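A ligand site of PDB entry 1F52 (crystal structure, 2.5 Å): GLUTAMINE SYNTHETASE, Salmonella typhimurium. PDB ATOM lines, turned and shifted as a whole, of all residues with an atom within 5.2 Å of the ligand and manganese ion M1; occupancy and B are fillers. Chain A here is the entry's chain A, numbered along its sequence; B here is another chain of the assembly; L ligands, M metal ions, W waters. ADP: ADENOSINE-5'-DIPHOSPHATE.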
ATOM      1  N   LEU A 125       0.107  26.203  15.970  1.00  0.00           N
ATOM      2  CA  LEU A 125       1.495  26.056  16.365  1.00  0.00           C
ATOM      3  C   LEU A 125       2.166  24.831  15.789  1.00  0.00           C
ATOM      4  O   LEU A 125       1.682  23.700  15.960  1.00  0.00           O
ATOM      5  CB  LEU A 125       1.602  26.064  17.878  1.00  0.00           C
ATOM      6  CG  LEU A 125       1.895  27.419  18.527  1.00  0.00           C
ATOM      7  CD1 LEU A 125       1.437  28.574  17.658  1.00  0.00           C
ATOM      8  CD2 LEU A 125       1.250  27.445  19.877  1.00  0.00           C
ATOM      9  N   PHE A 126       3.277  25.049  15.089  1.00  0.00           N
ATOM     10  CA  PHE A 126       4.051  23.974  14.475  1.00  0.00           C
ATOM     11  C   PHE A 126       5.458  23.878  15.006  1.00  0.00           C
ATOM     12  O   PHE A 126       6.195  24.879  15.072  1.00  0.00           O
ATOM     13  CB  PHE A 126       4.115  24.152  12.967  1.00  0.00           C
ATOM     14  CG  PHE A 126       2.988  23.489  12.247  1.00  0.00           C
ATOM     15  CD1 PHE A 126       1.750  24.102  12.151  1.00  0.00           C
ATOM     16  CD2 PHE A 126       3.168  22.240  11.646  1.00  0.00           C
ATOM     17  CE1 PHE A 126       0.699  23.490  11.472  1.00  0.00           C
ATOM     18  CE2 PHE A 126       2.129  21.616  10.969  1.00  0.00           C
ATOM     19  CZ  PHE A 126       0.900  22.237  10.879  1.00  0.00           C
ATOM     20  N   GLY A 127       5.826  22.669  15.398  1.00  0.00           N
ATOM     21  CA  GLY A 127       7.158  22.407  15.890  1.00  0.00           C
ATOM     22  C   GLY A 127       7.721  21.210  15.147  1.00  0.00           C
ATOM     23  O   GLY A 127       7.650  20.082  15.648  1.00  0.00           O
ATOM     24  N   PRO A 128       8.214  21.406  13.916  1.00  0.00           N
ATOM     25  CA  PRO A 128       8.774  20.303  13.130  1.00  0.00           C
ATOM     26  C   PRO A 128      10.203  19.979  13.566  1.00  0.00           C
ATOM     27  O   PRO A 128      10.919  20.842  14.069  1.00  0.00           O
ATOM     28  CB  PRO A 128       8.710  20.847  11.719  1.00  0.00           C
ATOM     29  CG  PRO A 128       8.999  22.291  11.911  1.00  0.00           C
ATOM     30  CD  PRO A 128       8.202  22.656  13.140  1.00  0.00           C
ATOM     31  N   GLU A 129      10.599  18.720  13.408  1.00  0.00           N
ATOM     32  CA  GLU A 129      11.930  18.272  13.813  1.00  0.00           C
ATOM     33  C   GLU A 129      12.656  17.654  12.630  1.00  0.00           C
ATOM     34  O   GLU A 129      12.767  16.434  12.520  1.00  0.00           O
ATOM     35  CB  GLU A 129      11.799  17.230  14.931  1.00  0.00           C
ATOM     36  CG  GLU A 129      10.887  17.689  16.056  1.00  0.00           C
ATOM     37  CD  GLU A 129      10.595  16.624  17.101  1.00  0.00           C
ATOM     38  OE1 GLU A 129      10.753  16.984  18.281  1.00  0.00           O
ATOM     39  OE2 GLU A 129      10.208  15.480  16.779  1.00  0.00           O
ATOM     40  N   GLU A 207      16.724  24.785  20.503  1.00  0.00           N
ATOM     41  CA  GLU A 207      16.477  24.095  21.756  1.00  0.00           C
ATOM     42  C   GLU A 207      17.539  23.047  22.063  1.00  0.00           C
ATOM     43  O   GLU A 207      17.873  22.813  23.224  1.00  0.00           O
ATOM     44  CB  GLU A 207      15.074  23.504  21.780  1.00  0.00           C
ATOM     45  CG  GLU A 207      14.032  24.604  21.658  1.00  0.00           C
ATOM     46  CD  GLU A 207      12.611  24.131  21.857  1.00  0.00           C
ATOM     47  OE1 GLU A 207      12.296  23.023  21.379  1.00  0.00           O
ATOM     48  OE2 GLU A 207      11.817  24.848  22.497  1.00  0.00           O
ATOM     49  N   GLU A 220      20.915  16.344  13.952  1.00  0.00           N
ATOM     50  CA  GLU A 220      19.671  17.092  14.143  1.00  0.00           C
ATOM     51  C   GLU A 220      19.841  18.340  14.989  1.00  0.00           C
ATOM     52  O   GLU A 220      20.501  18.312  16.027  1.00  0.00           O
ATOM     53  CB  GLU A 220      18.560  16.208  14.765  1.00  0.00           C
ATOM     54  CG  GLU A 220      17.221  16.906  14.980  1.00  0.00           C
ATOM     55  CD  GLU A 220      16.130  16.001  15.497  1.00  0.00           C
ATOM     56  OE1 GLU A 220      16.359  14.790  15.641  1.00  0.00           O
ATOM     57  OE2 GLU A 220      15.024  16.520  15.778  1.00  0.00           O
ATOM     58  N   ALA A 222      17.347  20.933  16.836  1.00  0.00           N
ATOM     59  CA  ALA A 222      15.977  21.154  17.252  1.00  0.00           C
ATOM     60  C   ALA A 222      15.713  22.611  17.529  1.00  0.00           C
ATOM     61  O   ALA A 222      16.422  23.248  18.302  1.00  0.00           O
ATOM     62  CB  ALA A 222      15.666  20.317  18.491  1.00  0.00           C
ATOM     63  N   THR A 223      14.698  23.137  16.870  1.00  0.00           N
ATOM     64  CA  THR A 223      14.337  24.536  17.029  1.00  0.00           C
ATOM     65  C   THR A 223      12.949  24.702  17.668  1.00  0.00           C
ATOM     66  O   THR A 223      12.109  23.811  17.557  1.00  0.00           O
ATOM     67  CB  THR A 223      14.356  25.259  15.689  1.00  0.00           C
ATOM     68  OG1 THR A 223      13.474  24.605  14.785  1.00  0.00           O
ATOM     69  CG2 THR A 223      15.767  25.258  15.118  1.00  0.00           C
ATOM     70  N   ARG A 224      12.723  25.840  18.328  1.00  0.00           N
ATOM     71  CA  ARG A 224      11.442  26.138  18.953  1.00  0.00           C
ATOM     72  C   ARG A 224      10.370  26.339  17.901  1.00  0.00           C
ATOM     73  O   ARG A 224      10.610  26.860  16.825  1.00  0.00           O
ATOM     74  CB  ARG A 224      11.555  27.365  19.853  1.00  0.00           C
ATOM     75  CG  ARG A 224      10.327  27.612  20.720  1.00  0.00           C
ATOM     76  CD  ARG A 224      10.231  29.063  21.160  1.00  0.00           C
ATOM     77  NE  ARG A 224      10.195  29.976  20.028  1.00  0.00           N
ATOM     78  CZ  ARG A 224       9.806  31.237  20.101  1.00  0.00           C
ATOM     79  NH1 ARG A 224       9.413  31.748  21.267  1.00  0.00           N
ATOM     80  NH2 ARG A 224       9.798  32.003  19.019  1.00  0.00           N
ATOM     81  N   PHE A 225       9.161  25.903  18.278  1.00  0.00           N
ATOM     82  CA  PHE A 225       7.997  25.990  17.402  1.00  0.00           C
ATOM     83  C   PHE A 225       7.735  27.459  17.127  1.00  0.00           C
ATOM     84  O   PHE A 225       8.430  28.328  17.636  1.00  0.00           O
ATOM     85  CB  PHE A 225       6.745  25.413  18.116  1.00  0.00           C
ATOM     86  CG  PHE A 225       6.383  26.281  19.292  1.00  0.00           C
ATOM     87  CD1 PHE A 225       6.961  26.050  20.527  1.00  0.00           C
ATOM     88  CD2 PHE A 225       5.515  27.363  19.162  1.00  0.00           C
ATOM     89  CE1 PHE A 225       6.700  26.893  21.598  1.00  0.00           C
ATOM     90  CE2 PHE A 225       5.243  28.210  20.225  1.00  0.00           C
ATOM     91  CZ  PHE A 225       5.840  27.980  21.446  1.00  0.00           C
ATOM     92  N   HIS A 269       9.215  14.982  12.241  1.00  0.00           N
ATOM     93  CA  HIS A 269       8.051  14.926  13.103  1.00  0.00           C
ATOM     94  C   HIS A 269       7.468  16.309  13.225  1.00  0.00           C
ATOM     95  O   HIS A 269       8.197  17.298  13.307  1.00  0.00           O
ATOM     96  CB  HIS A 269       8.453  14.506  14.506  1.00  0.00           C
ATOM     97  CG  HIS A 269       9.049  13.150  14.602  1.00  0.00           C
ATOM     98  ND1 HIS A 269       9.660  12.687  15.750  1.00  0.00           N
ATOM     99  CD2 HIS A 269       9.115  12.124  13.705  1.00  0.00           C
ATOM    100  CE1 HIS A 269      10.073  11.454  15.559  1.00  0.00           C
ATOM    101  NE2 HIS A 269       9.752  11.089  14.331  1.00  0.00           N
ATOM    102  N   HIS A 271       5.018  18.570  15.608  1.00  0.00           N
ATOM    103  CA  HIS A 271       4.265  18.801  16.821  1.00  0.00           C
ATOM    104  C   HIS A 271       3.296  19.911  16.474  1.00  0.00           C
ATOM    105  O   HIS A 271       3.679  20.904  15.839  1.00  0.00           O
ATOM    106  CB  HIS A 271       5.187  19.248  17.942  1.00  0.00           C
ATOM    107  CG  HIS A 271       6.096  18.185  18.454  1.00  0.00           C
ATOM    108  ND1 HIS A 271       6.240  17.905  19.789  1.00  0.00           N
ATOM    109  CD2 HIS A 271       6.907  17.311  17.809  1.00  0.00           C
ATOM    110  CE1 HIS A 271       7.090  16.911  19.948  1.00  0.00           C
ATOM    111  NE2 HIS A 271       7.507  16.530  18.762  1.00  0.00           N
ATOM    112  N   MET A 272       2.029  19.735  16.849  1.00  0.00           N
ATOM    113  CA  MET A 272       1.014  20.735  16.576  1.00  0.00           C
ATOM    114  C   MET A 272       0.061  20.944  17.746  1.00  0.00           C
ATOM    115  O   MET A 272      -0.117  20.064  18.590  1.00  0.00           O
ATOM    116  CB  MET A 272       0.195  20.330  15.362  1.00  0.00           C
ATOM    117  CG  MET A 272       0.959  20.333  14.070  1.00  0.00           C
ATOM    118  SD  MET A 272       0.015  19.504  12.822  1.00  0.00           S
ATOM    119  CE  MET A 272      -0.003  17.860  13.486  1.00  0.00           C
ATOM    120  N   SER A 273      -0.561  22.115  17.778  1.00  0.00           N
ATOM    121  CA  SER A 273      -1.527  22.487  18.795  1.00  0.00           C
ATOM    122  C   SER A 273      -2.195  23.756  18.319  1.00  0.00           C
ATOM    123  O   SER A 273      -1.637  24.481  17.493  1.00  0.00           O
ATOM    124  CB  SER A 273      -0.866  22.723  20.151  1.00  0.00           C
ATOM    125  OG  SER A 273      -0.123  23.924  20.151  1.00  0.00           O
ATOM    126  N   ASN A 280      -4.350  27.226  25.428  1.00  0.00           N
ATOM    127  CA  ASN A 280      -4.105  26.049  24.587  1.00  0.00           C
ATOM    128  C   ASN A 280      -5.345  25.192  24.385  1.00  0.00           C
ATOM    129  O   ASN A 280      -5.666  24.328  25.207  1.00  0.00           O
ATOM    130  CB  ASN A 280      -2.966  25.213  25.191  1.00  0.00           C
ATOM    131  CG  ASN A 280      -2.472  24.122  24.247  1.00  0.00           C
ATOM    132  OD1 ASN A 280      -3.171  23.713  23.304  1.00  0.00           O
ATOM    133  ND2 ASN A 280      -1.264  23.643  24.495  1.00  0.00           N
ATOM    134  N   ARG A 339       5.565   3.655  20.160  1.00  0.00           N
ATOM    135  CA  ARG A 339       6.249   4.349  19.072  1.00  0.00           C
ATOM    136  C   ARG A 339       6.184   3.563  17.768  1.00  0.00           C
ATOM    137  O   ARG A 339       7.174   3.420  17.053  1.00  0.00           O
ATOM    138  CB  ARG A 339       7.683   4.780  19.451  1.00  0.00           C
ATOM    139  CG  ARG A 339       7.757   6.073  20.291  1.00  0.00           C
ATOM    140  CD  ARG A 339       9.191   6.604  20.382  1.00  0.00           C
ATOM    141  NE  ARG A 339       9.374   7.687  21.368  1.00  0.00           N
ATOM    142  CZ  ARG A 339      10.123   8.775  21.185  1.00  0.00           C
ATOM    143  NH1 ARG A 339      10.251   9.708  22.129  1.00  0.00           N
ATOM    144  NH2 ARG A 339      10.739   8.974  20.016  1.00  0.00           N
ATOM    145  N   ARG A 344       2.171  10.461  18.150  1.00  0.00           N
ATOM    146  CA  ARG A 344       2.539  10.355  19.562  1.00  0.00           C
ATOM    147  C   ARG A 344       1.925  11.487  20.337  1.00  0.00           C
ATOM    148  O   ARG A 344       1.755  12.600  19.828  1.00  0.00           O
ATOM    149  CB  ARG A 344       4.035  10.386  19.864  1.00  0.00           C
ATOM    150  CG  ARG A 344       4.287   9.978  21.317  1.00  0.00           C
ATOM    151  CD  ARG A 344       5.748   9.672  21.564  1.00  0.00           C
ATOM    152  NE  ARG A 344       6.567  10.789  21.132  1.00  0.00           N
ATOM    153  CZ  ARG A 344       6.698  11.958  21.726  1.00  0.00           C
ATOM    154  NH1 ARG A 344       6.044  12.182  22.860  1.00  0.00           N
ATOM    155  NH2 ARG A 344       7.463  12.895  21.194  1.00  0.00           N
ATOM    156  N   LYS A 352      -0.245  23.903  29.340  1.00  0.00           N
ATOM    157  CA  LYS A 352       0.042  24.939  28.349  1.00  0.00           C
ATOM    158  C   LYS A 352       0.843  24.376  27.185  1.00  0.00           C
ATOM    159  O   LYS A 352       0.828  24.929  26.086  1.00  0.00           O
ATOM    160  CB  LYS A 352       0.811  26.091  29.008  1.00  0.00           C
ATOM    161  CG  LYS A 352       0.017  26.836  30.080  1.00  0.00           C
ATOM    162  CD  LYS A 352       0.793  27.998  30.658  1.00  0.00           C
ATOM    163  CE  LYS A 352      -0.041  28.735  31.703  1.00  0.00           C
ATOM    164  NZ  LYS A 352       0.713  29.832  32.348  1.00  0.00           N
ATOM    165  N   ALA A 353       1.500  23.242  27.426  1.00  0.00           N
ATOM    166  CA  ALA A 353       2.336  22.585  26.426  1.00  0.00           C
ATOM    167  C   ALA A 353       1.746  21.298  25.835  1.00  0.00           C
ATOM    168  O   ALA A 353       2.464  20.535  25.182  1.00  0.00           O
ATOM    169  CB  ALA A 353       3.715  22.301  27.021  1.00  0.00           C
ATOM    170  N   ARG A 354       0.461  21.053  26.049  1.00  0.00           N
ATOM    171  CA  ARG A 354      -0.198  19.853  25.518  1.00  0.00           C
ATOM    172  C   ARG A 354      -0.292  19.995  23.988  1.00  0.00           C
ATOM    173  O   ARG A 354      -0.667  21.055  23.476  1.00  0.00           O
ATOM    174  CB  ARG A 354      -1.604  19.725  26.130  1.00  0.00           C
ATOM    175  CG  ARG A 354      -2.082  18.287  26.362  1.00  0.00           C
ATOM    176  CD  ARG A 354      -1.552  17.687  27.668  1.00  0.00           C
ATOM    177  NE  ARG A 354      -2.227  18.211  28.850  1.00  0.00           N
ATOM    178  CZ  ARG A 354      -1.729  18.158  30.088  1.00  0.00           C
ATOM    179  NH1 ARG A 354      -2.417  18.664  31.109  1.00  0.00           N
ATOM    180  NH2 ARG A 354      -0.545  17.615  30.303  1.00  0.00           N
ATOM    181  N   ARG A 355       0.015  18.922  23.266  1.00  0.00           N
ATOM    182  CA  ARG A 355       0.008  18.939  21.798  1.00  0.00           C
ATOM    183  C   ARG A 355       0.086  17.522  21.210  1.00  0.00           C
ATOM    184  O   ARG A 355       0.196  16.552  21.956  1.00  0.00           O
ATOM    185  CB  ARG A 355       1.246  19.712  21.341  1.00  0.00           C
ATOM    186  CG  ARG A 355       2.536  19.012  21.778  1.00  0.00           C
ATOM    187  CD  ARG A 355       3.692  19.975  21.930  1.00  0.00           C
ATOM    188  NE  ARG A 355       4.938  19.249  22.179  1.00  0.00           N
ATOM    189  CZ  ARG A 355       5.657  19.339  23.285  1.00  0.00           C
ATOM    190  NH1 ARG A 355       6.775  18.637  23.404  1.00  0.00           N
ATOM    191  NH2 ARG A 355       5.280  20.122  24.288  1.00  0.00           N
ATOM    192  N   GLU A 357       2.002  14.898  18.160  1.00  0.00           N
ATOM    193  CA  GLU A 357       3.165  14.780  17.295  1.00  0.00           C
ATOM    194  C   GLU A 357       2.903  13.823  16.150  1.00  0.00           C
ATOM    195  O   GLU A 357       2.781  12.623  16.354  1.00  0.00           O
ATOM    196  CB  GLU A 357       4.393  14.283  18.075  1.00  0.00           C
ATOM    197  CG  GLU A 357       5.627  14.252  17.203  1.00  0.00           C
ATOM    198  CD  GLU A 357       6.804  13.521  17.805  1.00  0.00           C
ATOM    199  OE1 GLU A 357       6.610  12.420  18.339  1.00  0.00           O
ATOM    200  OE2 GLU A 357       7.933  14.016  17.692  1.00  0.00           O
ATOM    201  N   ARG A 359       4.245  11.911  13.351  1.00  0.00           N
ATOM    202  CA  ARG A 359       5.568  11.420  13.041  1.00  0.00           C
ATOM    203  C   ARG A 359       5.945  11.059  11.588  1.00  0.00           C
ATOM    204  O   ARG A 359       7.133  10.888  11.303  1.00  0.00           O
ATOM    205  CB  ARG A 359       5.754  10.166  13.893  1.00  0.00           C
ATOM    206  CG  ARG A 359       5.075  10.131  15.239  1.00  0.00           C
ATOM    207  CD  ARG A 359       6.126  10.477  16.258  1.00  0.00           C
ATOM    208  NE  ARG A 359       7.127   9.449  16.313  1.00  0.00           N
ATOM    209  CZ  ARG A 359       8.077   9.493  17.222  1.00  0.00           C
ATOM    210  NH1 ARG A 359       8.086  10.481  18.096  1.00  0.00           N
ATOM    211  NH2 ARG A 359       9.037   8.566  17.256  1.00  0.00           N
ATOM    212  N   MET B  48      13.530  16.225  29.005  1.00  0.00           N
ATOM    213  CA  MET B  48      13.001  14.952  28.504  1.00  0.00           C
ATOM    214  C   MET B  48      13.745  14.432  27.292  1.00  0.00           C
ATOM    215  O   MET B  48      14.176  15.201  26.425  1.00  0.00           O
ATOM    216  CB  MET B  48      11.540  15.126  28.099  1.00  0.00           C
ATOM    217  CG  MET B  48      10.598  15.320  29.257  1.00  0.00           C
ATOM    218  SD  MET B  48      10.463  13.813  30.209  1.00  0.00           S
ATOM    219  CE  MET B  48       8.997  13.117  29.477  1.00  0.00           C
HETATM  220  PB  ADP L   1      11.051  14.779  20.291  1.00  0.00           P
HETATM  221  O1B ADP L   1      11.828  13.968  21.340  1.00  0.00           O
HETATM  222  O2B ADP L   1       9.662  14.331  20.007  1.00  0.00           O
HETATM  223  O3B ADP L   1      11.988  14.831  18.904  1.00  0.00           O
HETATM  224  PA  ADP L   1      12.153  17.654  20.956  1.00  0.00           P
HETATM  225  O1A ADP L   1      13.207  17.530  22.053  1.00  0.00           O
HETATM  226  O2A ADP L   1      12.875  17.825  19.568  1.00  0.00           O
HETATM  227  O3A ADP L   1      11.100  16.329  20.900  1.00  0.00           O
HETATM  228  O5' ADP L   1      11.362  19.067  21.297  1.00  0.00           O
HETATM  229  C5' ADP L   1      10.790  20.137  20.614  1.00  0.00           C
HETATM  230  C4' ADP L   1       9.569  20.383  19.787  1.00  0.00           C
HETATM  231  O4' ADP L   1       8.144  20.440  20.450  1.00  0.00           O
HETATM  232  C3' ADP L   1       9.815  21.770  19.395  1.00  0.00           C
HETATM  233  O3' ADP L   1       9.634  21.829  18.001  1.00  0.00           O
HETATM  234  C2' ADP L   1       8.797  22.504  20.321  1.00  0.00           C
HETATM  235  O2' ADP L   1       8.878  23.894  20.124  1.00  0.00           O
HETATM  236  C1' ADP L   1       7.628  21.731  19.812  1.00  0.00           C
HETATM  237  N9  ADP L   1       6.114  22.330  20.172  1.00  0.00           N
HETATM  238  C8  ADP L   1       5.003  22.373  19.245  1.00  0.00           C
HETATM  239  N7  ADP L   1       3.829  22.898  19.626  1.00  0.00           N
HETATM  240  C5  ADP L   1       4.127  23.215  20.933  1.00  0.00           C
HETATM  241  C6  ADP L   1       3.310  23.778  21.911  1.00  0.00           C
HETATM  242  N6  ADP L   1       2.172  24.060  21.599  1.00  0.00           N
HETATM  243  N1  ADP L   1       3.784  24.033  23.153  1.00  0.00           N
HETATM  244  C2  ADP L   1       5.069  23.700  23.449  1.00  0.00           C
HETATM  245  N3  ADP L   1       6.022  23.133  22.627  1.00  0.00           N
HETATM  246  C4  ADP L   1       5.485  22.885  21.335  1.00  0.00           C
HETATM  247 MN    MN M   1      10.096  13.687  17.767  1.00  0.00          MN
HETATM  248 MN    MN M   2      15.362  12.985  15.986  1.00  0.00          MN
HETATM  249  O   HOH W   1      10.307  23.353  15.307  1.00  0.00           O
HETATM  250  O   HOH W   2      12.655  12.961  17.532  1.00  0.00           O
HETATM  251  O   HOH W   3      14.951  15.549  18.673  1.00  0.00           O
HETATM  252  O   HOH W   4      11.311  14.249  24.144  1.00  0.00           O
HETATM  253  O   HOH W   5       9.996  12.063  19.116  1.00  0.00           O
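NE2 of His 271 touches manganese ion M1 (3.97 Å).
Arg 359 touches manganese ion M1 (NH1 to MN, 3.8 Å).
Five residues have an atom within 4 Å of manganese ion M1: Glu 129, His 269, His 271, Glu 357 and Arg 359.
The nearest printed residue that does not touch manganese ion M1 is Arg 344 (4.4 Å).
The side-chain carboxylate of Glu 357 is in salt-bridge range of the guanidinium group of Arg 344, 3.0 Å away.
The backbone carbonyl oxygen of Ser 273 sits at hydrogen-bond distance from the backbone NH of Leu 125.
The side-chain carboxylate (OE2) of Glu 357 lies close to a ring nitrogen (NE2) of His 271, 2.8 Å away.
The backbone NH of Gly 127 sits at hydrogen-bond distance from the backbone carbonyl oxygen of His 271.
The backbone carbonyl oxygen (O) of Ala 222 sits at hydrogen-bond distance from the backbone NH (N) of Glu 207.
The side-chain carboxylate (OE1) of Glu 129 is in hydrogen-bond range of a ring nitrogen (NE2) of His 271, 3.3 Å away.
The guanidinium group (NE) of Arg 355 is in hydrogen-bond range of a ring nitrogen (ND1) of His 271.
NH1 of Arg 359 lies within salt-bridge range of OE1 of Glu 357.
Water W3 lies within hydrogen-bond range of OE2 of Glu 220 and O2A of the ligand.
Water W1 lies within hydrogen-bond range of O of Pro 128, O of Thr 223 and O3' of the ligand.
Leu 125 touches the ligand.
Gly 127 touches the ligand.
Glu 207 touches the ligand (OE1 to C5', 3.3 Å).
Ala 222 touches the ligand.
Arg 224 touches the ligand (CA to O2', 3.6 Å).
CA of Ala 353 touches N1 of the ligand, 3.9 Å away.
Arg 355 touches the ligand (CD to C5, 3.4 Å).
Within 4 Å of the ligand: Leu 125, Gly 127, Glu 129, Glu 207, Ala 222, Thr 223, Arg 224, Phe 225, His 271, Ser 273, Arg 344, Ala 353, Arg 355 and Glu 357.
The nearest printed residue that does not touch the ligand is Pro 128 (4.3 Å).
Manganese ion M1 is bound by OE2 of Glu 129 (2.1 Å), water W5 (2.1 Å), OE2 of Glu 357 (2.2 Å), ND1 of His 269 (2.3 Å), O2B of the ligand (2.4 Å), O3B of the ligand (2.5 Å) and water W2 (2.7 Å).
An oxygen (O4') of the ligand lies within hydrogen-bond range of a ring nitrogen (ND1) of His 271 (3.2 Å).
The backbone carbonyl oxygen (O) of Thr 223 is in hydrogen-bond range of an oxygen (O3') of the ligand (3.2 Å).
A nitrogen (N6) of the ligand is in hydrogen-bond range of the side-chain hydroxyl (OG) of Ser 273 (2.7 Å).
N of Phe 225 is in hydrogen-bond range of O2' of the ligand (2.7 Å).
O2B of the ligand lies close to NH2 of Arg 344.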
